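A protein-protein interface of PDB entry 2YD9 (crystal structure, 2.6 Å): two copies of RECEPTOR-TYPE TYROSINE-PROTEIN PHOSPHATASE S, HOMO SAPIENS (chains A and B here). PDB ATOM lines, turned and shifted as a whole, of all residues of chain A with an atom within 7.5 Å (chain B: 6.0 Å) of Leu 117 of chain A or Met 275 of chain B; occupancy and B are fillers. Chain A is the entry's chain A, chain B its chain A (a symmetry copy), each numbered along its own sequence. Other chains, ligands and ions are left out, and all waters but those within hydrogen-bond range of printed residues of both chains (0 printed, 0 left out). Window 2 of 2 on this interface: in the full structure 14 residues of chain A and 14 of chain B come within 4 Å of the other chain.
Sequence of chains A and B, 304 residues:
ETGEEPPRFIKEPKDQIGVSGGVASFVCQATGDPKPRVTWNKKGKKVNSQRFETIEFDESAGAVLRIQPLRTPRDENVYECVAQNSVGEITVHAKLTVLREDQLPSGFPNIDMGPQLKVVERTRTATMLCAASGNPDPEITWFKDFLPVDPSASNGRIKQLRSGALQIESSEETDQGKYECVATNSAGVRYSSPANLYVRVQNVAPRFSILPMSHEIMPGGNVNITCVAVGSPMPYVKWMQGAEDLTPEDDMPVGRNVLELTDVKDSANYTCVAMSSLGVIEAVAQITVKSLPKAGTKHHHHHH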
ATOM      1  N   GLY A 114      10.387  13.754  34.969  1.00  0.00           N
ATOM      2  CA  GLY A 114      11.426  14.776  35.042  1.00  0.00           C
ATOM      3  C   GLY A 114      12.547  14.515  34.052  1.00  0.00           C
ATOM      4  O   GLY A 114      12.541  13.501  33.354  1.00  0.00           O
ATOM      5  N   PRO A 115      13.530  15.429  33.996  1.00  0.00           N
ATOM      6  CA  PRO A 115      14.674  15.264  33.111  1.00  0.00           C
ATOM      7  C   PRO A 115      15.653  14.227  33.649  1.00  0.00           C
ATOM      8  O   PRO A 115      15.601  13.883  34.825  1.00  0.00           O
ATOM      9  CB  PRO A 115      15.305  16.652  33.107  1.00  0.00           C
ATOM     10  CG  PRO A 115      14.989  17.194  34.441  1.00  0.00           C
ATOM     11  CD  PRO A 115      13.635  16.665  34.792  1.00  0.00           C
ATOM     12  N   GLN A 116      16.544  13.758  32.782  1.00  0.00           N
ATOM     13  CA  GLN A 116      17.467  12.676  33.096  1.00  0.00           C
ATOM     14  C   GLN A 116      18.833  12.957  32.506  1.00  0.00           C
ATOM     15  O   GLN A 116      18.949  13.672  31.513  1.00  0.00           O
ATOM     16  CB  GLN A 116      16.958  11.361  32.516  1.00  0.00           C
ATOM     17  CG  GLN A 116      16.017  10.600  33.426  1.00  0.00           C
ATOM     18  CD  GLN A 116      15.424   9.378  32.743  1.00  0.00           C
ATOM     19  OE1 GLN A 116      15.679   9.120  31.562  1.00  0.00           O
ATOM     20  NE2 GLN A 116      14.625   8.620  33.485  1.00  0.00           N
ATOM     21  N   LEU A 117      19.858  12.375  33.121  1.00  0.00           N
ATOM     22  CA  LEU A 117      21.222  12.424  32.610  1.00  0.00           C
ATOM     23  C   LEU A 117      21.211  12.288  31.097  1.00  0.00           C
ATOM     24  O   LEU A 117      20.628  11.339  30.570  1.00  0.00           O
ATOM     25  CB  LEU A 117      22.053  11.294  33.229  1.00  0.00           C
ATOM     26  CG  LEU A 117      23.396  10.932  32.584  1.00  0.00           C
ATOM     27  CD1 LEU A 117      24.219  12.164  32.270  1.00  0.00           C
ATOM     28  CD2 LEU A 117      24.175   9.997  33.493  1.00  0.00           C
ATOM     29  N   LYS A 118      21.847  13.231  30.405  1.00  0.00           N
ATOM     30  CA  LYS A 118      21.911  13.192  28.944  1.00  0.00           C
ATOM     31  C   LYS A 118      23.268  13.639  28.393  1.00  0.00           C
ATOM     32  O   LYS A 118      23.953  14.464  29.002  1.00  0.00           O
ATOM     33  CB  LYS A 118      20.807  14.068  28.370  1.00  0.00           C
ATOM     34  CG  LYS A 118      20.511  13.823  26.913  1.00  0.00           C
ATOM     35  CD  LYS A 118      19.378  14.706  26.422  1.00  0.00           C
ATOM     36  CE  LYS A 118      18.023  14.201  26.898  1.00  0.00           C
ATOM     37  NZ  LYS A 118      16.920  15.057  26.373  1.00  0.00           N
ATOM     38  N   VAL A 119      23.646  13.074  27.247  1.00  0.00           N
ATOM     39  CA  VAL A 119      24.808  13.534  26.481  1.00  0.00           C
ATOM     40  C   VAL A 119      24.329  14.028  25.129  1.00  0.00           C
ATOM     41  O   VAL A 119      23.528  13.372  24.475  1.00  0.00           O
ATOM     42  CB  VAL A 119      25.847  12.407  26.234  1.00  0.00           C
ATOM     43  CG1 VAL A 119      27.110  12.978  25.601  1.00  0.00           C
ATOM     44  CG2 VAL A 119      26.180  11.676  27.534  1.00  0.00           C
ATOM     45  N   GLU A 121      25.914  15.770  21.444  1.00  0.00           N
ATOM     46  CA  GLU A 121      27.108  16.183  20.707  1.00  0.00           C
ATOM     47  C   GLU A 121      26.962  17.662  20.361  1.00  0.00           C
ATOM     48  O   GLU A 121      25.845  18.163  20.264  1.00  0.00           O
ATOM     49  CB  GLU A 121      27.358  15.304  19.470  1.00  0.00           C
ATOM     50  CG  GLU A 121      28.164  14.017  19.774  1.00  0.00           C
ATOM     51  CD  GLU A 121      27.316  12.883  20.367  1.00  0.00           C
ATOM     52  OE1 GLU A 121      26.285  12.569  19.746  1.00  0.00           O
ATOM     53  OE2 GLU A 121      27.677  12.283  21.416  1.00  0.00           O
ATOM     54  N   MET A 128      15.471  18.789  27.247  1.00  0.00           N
ATOM     55  CA  MET A 128      15.302  18.348  28.629  1.00  0.00           C
ATOM     56  C   MET A 128      13.817  18.259  28.956  1.00  0.00           C
ATOM     57  O   MET A 128      13.166  19.274  29.179  1.00  0.00           O
ATOM     58  CB  MET A 128      15.994  19.317  29.594  1.00  0.00           C
ATOM     59  CG  MET A 128      17.425  19.653  29.214  1.00  0.00           C
ATOM     60  SD  MET A 128      18.490  18.213  29.085  1.00  0.00           S
ATOM     61  CE  MET A 128      18.590  17.720  30.805  1.00  0.00           C
ATOM     62  N   PRO A 194      17.461  16.353  39.863  1.00  0.00           N
ATOM     63  CA  PRO A 194      18.374  17.011  38.927  1.00  0.00           C
ATOM     64  C   PRO A 194      18.805  16.086  37.799  1.00  0.00           C
ATOM     65  O   PRO A 194      18.760  14.863  37.947  1.00  0.00           O
ATOM     66  CB  PRO A 194      19.592  17.364  39.790  1.00  0.00           C
ATOM     67  CG  PRO A 194      19.221  17.051  41.189  1.00  0.00           C
ATOM     68  CD  PRO A 194      18.110  16.072  41.151  1.00  0.00           C
ATOM     69  N   ALA A 195      19.229  16.667  36.685  1.00  0.00           N
ATOM     70  CA  ALA A 195      19.744  15.884  35.577  1.00  0.00           C
ATOM     71  C   ALA A 195      20.911  16.621  34.945  1.00  0.00           C
ATOM     72  O   ALA A 195      20.780  17.792  34.592  1.00  0.00           O
ATOM     73  CB  ALA A 195      18.639  15.631  34.545  1.00  0.00           C
ATOM     74  N   ASN A 196      22.051  15.943  34.821  1.00  0.00           N
ATOM     75  CA  ASN A 196      23.221  16.520  34.165  1.00  0.00           C
ATOM     76  C   ASN A 196      23.109  16.407  32.644  1.00  0.00           C
ATOM     77  O   ASN A 196      22.690  15.375  32.123  1.00  0.00           O
ATOM     78  CB  ASN A 196      24.499  15.836  34.641  1.00  0.00           C
ATOM     79  CG  ASN A 196      24.809  16.120  36.106  1.00  0.00           C
ATOM     80  OD1 ASN A 196      24.521  15.303  36.977  1.00  0.00           O
ATOM     81  ND2 ASN A 196      25.394  17.279  36.383  1.00  0.00           N
ATOM     82  N   LEU A 197      23.457  17.491  31.950  1.00  0.00           N
ATOM     83  CA  LEU A 197      23.607  17.491  30.495  1.00  0.00           C
ATOM     84  C   LEU A 197      25.099  17.587  30.174  1.00  0.00           C
ATOM     85  O   LEU A 197      25.781  18.474  30.687  1.00  0.00           O
ATOM     86  CB  LEU A 197      22.869  18.681  29.879  1.00  0.00           C
ATOM     87  CG  LEU A 197      22.903  18.783  28.347  1.00  0.00           C
ATOM     88  CD1 LEU A 197      22.126  17.628  27.706  1.00  0.00           C
ATOM     89  CD2 LEU A 197      22.358  20.126  27.867  1.00  0.00           C
ATOM     90  N   TYR A 198      25.606  16.669  29.355  1.00  0.00           N
ATOM     91  CA  TYR A 198      27.002  16.712  28.913  1.00  0.00           C
ATOM     92  C   TYR A 198      27.074  17.049  27.429  1.00  0.00           C
ATOM     93  O   TYR A 198      26.355  16.449  26.627  1.00  0.00           O
ATOM     94  CB  TYR A 198      27.683  15.370  29.191  1.00  0.00           C
ATOM     95  CG  TYR A 198      27.814  15.085  30.668  1.00  0.00           C
ATOM     96  CD1 TYR A 198      28.766  15.751  31.438  1.00  0.00           C
ATOM     97  CD2 TYR A 198      26.973  14.174  31.305  1.00  0.00           C
ATOM     98  CE1 TYR A 198      28.884  15.511  32.803  1.00  0.00           C
ATOM     99  CE2 TYR A 198      27.090  13.921  32.668  1.00  0.00           C
ATOM    100  CZ  TYR A 198      28.044  14.595  33.408  1.00  0.00           C
ATOM    101  OH  TYR A 198      28.164  14.350  34.752  1.00  0.00           O
ATOM    102  N   ARG A 200      29.269  16.951  24.179  1.00  0.00           N
ATOM    103  CA  ARG A 200      30.413  16.230  23.640  1.00  0.00           C
ATOM    104  C   ARG A 200      31.040  16.946  22.442  1.00  0.00           C
ATOM    105  O   ARG A 200      30.398  17.147  21.405  1.00  0.00           O
ATOM    106  CB  ARG A 200      29.980  14.816  23.230  1.00  0.00           C
ATOM    107  CG  ARG A 200      31.061  13.964  22.584  1.00  0.00           C
ATOM    108  CD  ARG A 200      31.859  13.231  23.613  1.00  0.00           C
ATOM    109  NE  ARG A 200      32.993  12.513  23.033  1.00  0.00           N
ATOM    110  CZ  ARG A 200      34.271  12.872  23.147  1.00  0.00           C
ATOM    111  NH1 ARG A 200      34.624  13.965  23.819  1.00  0.00           N
ATOM    112  NH2 ARG A 200      35.215  12.124  22.583  1.00  0.00           N
ATOM    113  N   PRO B 206      25.522   2.703  22.666  1.00  0.00           N
ATOM    114  CA  PRO B 206      26.670   2.250  23.424  1.00  0.00           C
ATOM    115  C   PRO B 206      26.438   0.912  24.114  1.00  0.00           C
ATOM    116  O   PRO B 206      25.348   0.666  24.625  1.00  0.00           O
ATOM    117  CB  PRO B 206      26.861   3.366  24.457  1.00  0.00           C
ATOM    118  CG  PRO B 206      25.513   3.908  24.680  1.00  0.00           C
ATOM    119  CD  PRO B 206      24.729   3.695  23.414  1.00  0.00           C
ATOM    120  N   MET B 234      31.388   7.455  20.474  1.00  0.00           N
ATOM    121  CA  MET B 234      32.027   6.653  21.508  1.00  0.00           C
ATOM    122  C   MET B 234      31.570   7.205  22.853  1.00  0.00           C
ATOM    123  O   MET B 234      31.629   8.413  23.073  1.00  0.00           O
ATOM    124  CB  MET B 234      33.543   6.760  21.367  1.00  0.00           C
ATOM    125  CG  MET B 234      34.317   5.601  21.948  1.00  0.00           C
ATOM    126  SD  MET B 234      34.227   4.122  20.926  1.00  0.00           S
ATOM    127  CE  MET B 234      35.335   3.030  21.820  1.00  0.00           C
ATOM    128  N   PRO B 235      31.108   6.334  23.761  1.00  0.00           N
ATOM    129  CA  PRO B 235      30.506   6.829  24.991  1.00  0.00           C
ATOM    130  C   PRO B 235      31.529   7.292  26.023  1.00  0.00           C
ATOM    131  O   PRO B 235      32.653   6.793  26.031  1.00  0.00           O
ATOM    132  CB  PRO B 235      29.776   5.596  25.524  1.00  0.00           C
ATOM    133  CG  PRO B 235      30.608   4.474  25.082  1.00  0.00           C
ATOM    134  CD  PRO B 235      31.153   4.862  23.739  1.00  0.00           C
ATOM    135  N   TYR B 236      31.137   8.240  26.876  1.00  0.00           N
ATOM    136  CA  TYR B 236      31.902   8.535  28.090  1.00  0.00           C
ATOM    137  C   TYR B 236      31.784   7.315  29.003  1.00  0.00           C
ATOM    138  O   TYR B 236      30.841   6.532  28.867  1.00  0.00           O
ATOM    139  CB  TYR B 236      31.338   9.743  28.835  1.00  0.00           C
ATOM    140  CG  TYR B 236      31.614  11.099  28.225  1.00  0.00           C
ATOM    141  CD1 TYR B 236      32.907  11.615  28.169  1.00  0.00           C
ATOM    142  CD2 TYR B 236      30.572  11.898  27.759  1.00  0.00           C
ATOM    143  CE1 TYR B 236      33.157  12.873  27.632  1.00  0.00           C
ATOM    144  CE2 TYR B 236      30.813  13.161  27.227  1.00  0.00           C
ATOM    145  CZ  TYR B 236      32.106  13.641  27.165  1.00  0.00           C
ATOM    146  OH  TYR B 236      32.339  14.895  26.637  1.00  0.00           O
ATOM    147  N   VAL B 237      32.725   7.157  29.930  1.00  0.00           N
ATOM    148  CA  VAL B 237      32.658   6.083  30.924  1.00  0.00           C
ATOM    149  C   VAL B 237      33.081   6.585  32.310  1.00  0.00           C
ATOM    150  O   VAL B 237      34.245   6.930  32.524  1.00  0.00           O
ATOM    151  CB  VAL B 237      33.535   4.896  30.506  1.00  0.00           C
ATOM    152  CG1 VAL B 237      33.584   3.853  31.607  1.00  0.00           C
ATOM    153  CG2 VAL B 237      33.010   4.286  29.215  1.00  0.00           C
ATOM    154  N   LYS B 238      32.124   6.623  33.239  1.00  0.00           N
ATOM    155  CA  LYS B 238      32.358   7.120  34.597  1.00  0.00           C
ATOM    156  C   LYS B 238      31.955   6.098  35.650  1.00  0.00           C
ATOM    157  O   LYS B 238      31.278   5.115  35.345  1.00  0.00           O
ATOM    158  CB  LYS B 238      31.587   8.419  34.835  1.00  0.00           C
ATOM    159  CG  LYS B 238      30.062   8.274  34.918  1.00  0.00           C
ATOM    160  CD  LYS B 238      29.421   9.572  35.405  1.00  0.00           C
ATOM    161  CE  LYS B 238      27.944   9.400  35.746  1.00  0.00           C
ATOM    162  NZ  LYS B 238      27.390  10.611  36.426  1.00  0.00           N
ATOM    163  N   MET B 252      36.564  13.518  31.961  1.00  0.00           N
ATOM    164  CA  MET B 252      35.877  12.239  32.013  1.00  0.00           C
ATOM    165  C   MET B 252      36.369  11.385  30.849  1.00  0.00           C
ATOM    166  O   MET B 252      36.346  11.838  29.705  1.00  0.00           O
ATOM    167  CB  MET B 252      34.369  12.452  31.914  1.00  0.00           C
ATOM    168  CG  MET B 252      33.556  11.214  32.243  1.00  0.00           C
ATOM    169  SD  MET B 252      31.814  11.569  32.524  1.00  0.00           S
ATOM    170  CE  MET B 252      31.897  12.583  34.001  1.00  0.00           C
ATOM    171  N   VAL B 273      28.985   3.423  34.581  1.00  0.00           N
ATOM    172  CA  VAL B 273      28.006   3.943  33.630  1.00  0.00           C
ATOM    173  C   VAL B 273      28.685   4.384  32.337  1.00  0.00           C
ATOM    174  O   VAL B 273      29.568   5.239  32.352  1.00  0.00           O
ATOM    175  CB  VAL B 273      27.198   5.117  34.207  1.00  0.00           C
ATOM    176  CG1 VAL B 273      26.039   5.451  33.283  1.00  0.00           C
ATOM    177  CG2 VAL B 273      26.687   4.781  35.596  1.00  0.00           C
ATOM    178  N   ALA B 274      28.271   3.771  31.231  1.00  0.00           N
ATOM    179  CA  ALA B 274      28.681   4.180  29.895  1.00  0.00           C
ATOM    180  C   ALA B 274      27.536   4.985  29.290  1.00  0.00           C
ATOM    181  O   ALA B 274      26.374   4.629  29.464  1.00  0.00           O
ATOM    182  CB  ALA B 274      28.999   2.967  29.048  1.00  0.00           C
ATOM    183  N   MET B 275      27.860   6.072  28.596  1.00  0.00           N
ATOM    184  CA  MET B 275      26.840   7.018  28.129  1.00  0.00           C
ATOM    185  C   MET B 275      27.240   7.789  26.876  1.00  0.00           C
ATOM    186  O   MET B 275      28.321   8.369  26.808  1.00  0.00           O
ATOM    187  CB  MET B 275      26.505   8.015  29.240  1.00  0.00           C
ATOM    188  CG  MET B 275      27.713   8.529  29.992  1.00  0.00           C
ATOM    189  SD  MET B 275      27.276   9.811  31.171  1.00  0.00           S
ATOM    190  CE  MET B 275      28.846  10.090  31.969  1.00  0.00           C
ATOM    191  N   SER B 276      26.345   7.782  25.892  1.00  0.00           N
ATOM    192  CA  SER B 276      26.490   8.582  24.681  1.00  0.00           C
ATOM    193  C   SER B 276      25.142   9.186  24.344  1.00  0.00           C
ATOM    194  O   SER B 276      24.157   8.959  25.047  1.00  0.00           O
ATOM    195  CB  SER B 276      26.989   7.718  23.516  1.00  0.00           C
ATOM    196  OG  SER B 276      26.024   6.766  23.095  1.00  0.00           O
ATOM    197  N   SER B 277      25.086   9.949  23.263  1.00  0.00           N
ATOM    198  CA  SER B 277      23.837  10.580  22.854  1.00  0.00           C
ATOM    199  C   SER B 277      22.788   9.559  22.401  1.00  0.00           C
ATOM    200  O   SER B 277      21.622   9.912  22.231  1.00  0.00           O
ATOM    201  CB  SER B 277      24.089  11.613  21.753  1.00  0.00           C
ATOM    202  OG  SER B 277      24.592  11.006  20.579  1.00  0.00           O
ATOM    203  N   GLY B 279      22.336   6.576  24.141  1.00  0.00           N
ATOM    204  CA  GLY B 279      21.904   5.800  25.302  1.00  0.00           C
ATOM    205  C   GLY B 279      22.825   5.805  26.507  1.00  0.00           C
ATOM    206  O   GLY B 279      23.965   6.282  26.448  1.00  0.00           O
ATOM    207  N   VAL B 280      22.299   5.270  27.608  1.00  0.00           N
ATOM    208  CA  VAL B 280      23.049   5.070  28.846  1.00  0.00           C
ATOM    209  C   VAL B 280      22.941   3.607  29.269  1.00  0.00           C
ATOM    210  O   VAL B 280      21.848   3.041  29.306  1.00  0.00           O
ATOM    211  CB  VAL B 280      22.517   5.968  29.981  1.00  0.00           C
ATOM    212  CG1 VAL B 280      23.262   5.695  31.280  1.00  0.00           C
ATOM    213  CG2 VAL B 280      22.646   7.431  29.591  1.00  0.00           C
ATOM    214  N   ILE B 281      24.078   3.005  29.585  1.00  0.00           N
ATOM    215  CA  ILE B 281      24.139   1.610  30.001  1.00  0.00           C
ATOM    216  C   ILE B 281      24.870   1.508  31.337  1.00  0.00           C
ATOM    217  O   ILE B 281      25.713   2.351  31.665  1.00  0.00           O
ATOM    218  CB  ILE B 281      24.856   0.729  28.947  1.00  0.00           C
ATOM    219  CG1 ILE B 281      26.150   1.398  28.470  1.00  0.00           C
ATOM    220  CG2 ILE B 281      23.939   0.465  27.766  1.00  0.00           C
ATOM    221  CD1 ILE B 281      27.082   0.476  27.731  1.00  0.00           C
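No position is printed for both chains.
Of the 5 pairs that touch across the chains among the printed residues, none has its exchanged pair printed and touching as well.
Of the 15 printed residues of chain B, 4 touch a printed residue of chain A.
Hydrophobic or aromatic side chains of chain A that line the printed part of chain B: Leu 117 and Val 119.
Among the printed residues, 5 pairs touch across the chains.
Among the printed residues, no Asp or Glu carboxylate lies within 4 Å of a Lys or Arg side-chain nitrogen of the other chain.
Leu 117 of chain A touches Met 275 of chain B.
Val 119 of chain A touches Ser 276 of chain B.
Ser 277 of chain B touches Val 119 of chain A.
CD of Arg 200 of chain A touches OH of Tyr 236 of chain B, 3.5 Å away.
The backbone NH of Tyr 236 of chain B sits at hydrogen-bond distance from the backbone carbonyl oxygen of Met 275 of chain B, 2.8 Å away.
The side-chain hydroxyl (OG) of Ser 277 of chain B lies within hydrogen-bond range of the side-chain carboxylate (OE1) of Glu 121 of chain A, 2.5 Å away.
Of chain B, only Met 275 comes within 4 Å of Leu 117 of chain A.
Printed residues of chain A within 4 Å of Met 275 of chain B: Leu 117.
Printed residues of chain A within 4 Å of Ser 276 of chain B: Val 119.
Printed residues of chain B within 4 Å of Arg 200 of chain A: Tyr 236.
Of the printed residues of chain A, Ser 277 of chain B touches Val 119 and Glu 121.
Printed residues of chain B within 4 Å of Val 119 of chain A: Ser 276 and Ser 277.
Of the printed residues of chain A, Tyr 236 of chain B touches Arg 200 (3.5 Å).
Val 280 of chain B touches none of the printed residues of chain A.
Pro 206 of chain B touches none of the printed residues of chain A.
The nearest residue of chain B that does not touch Leu 117 of chain A is Lys 238 of chain B (4.4 Å).
The nearest printed residue of chain A that does not touch Ser 277 of chain B is Lys 118 of chain A (6.2 Å).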
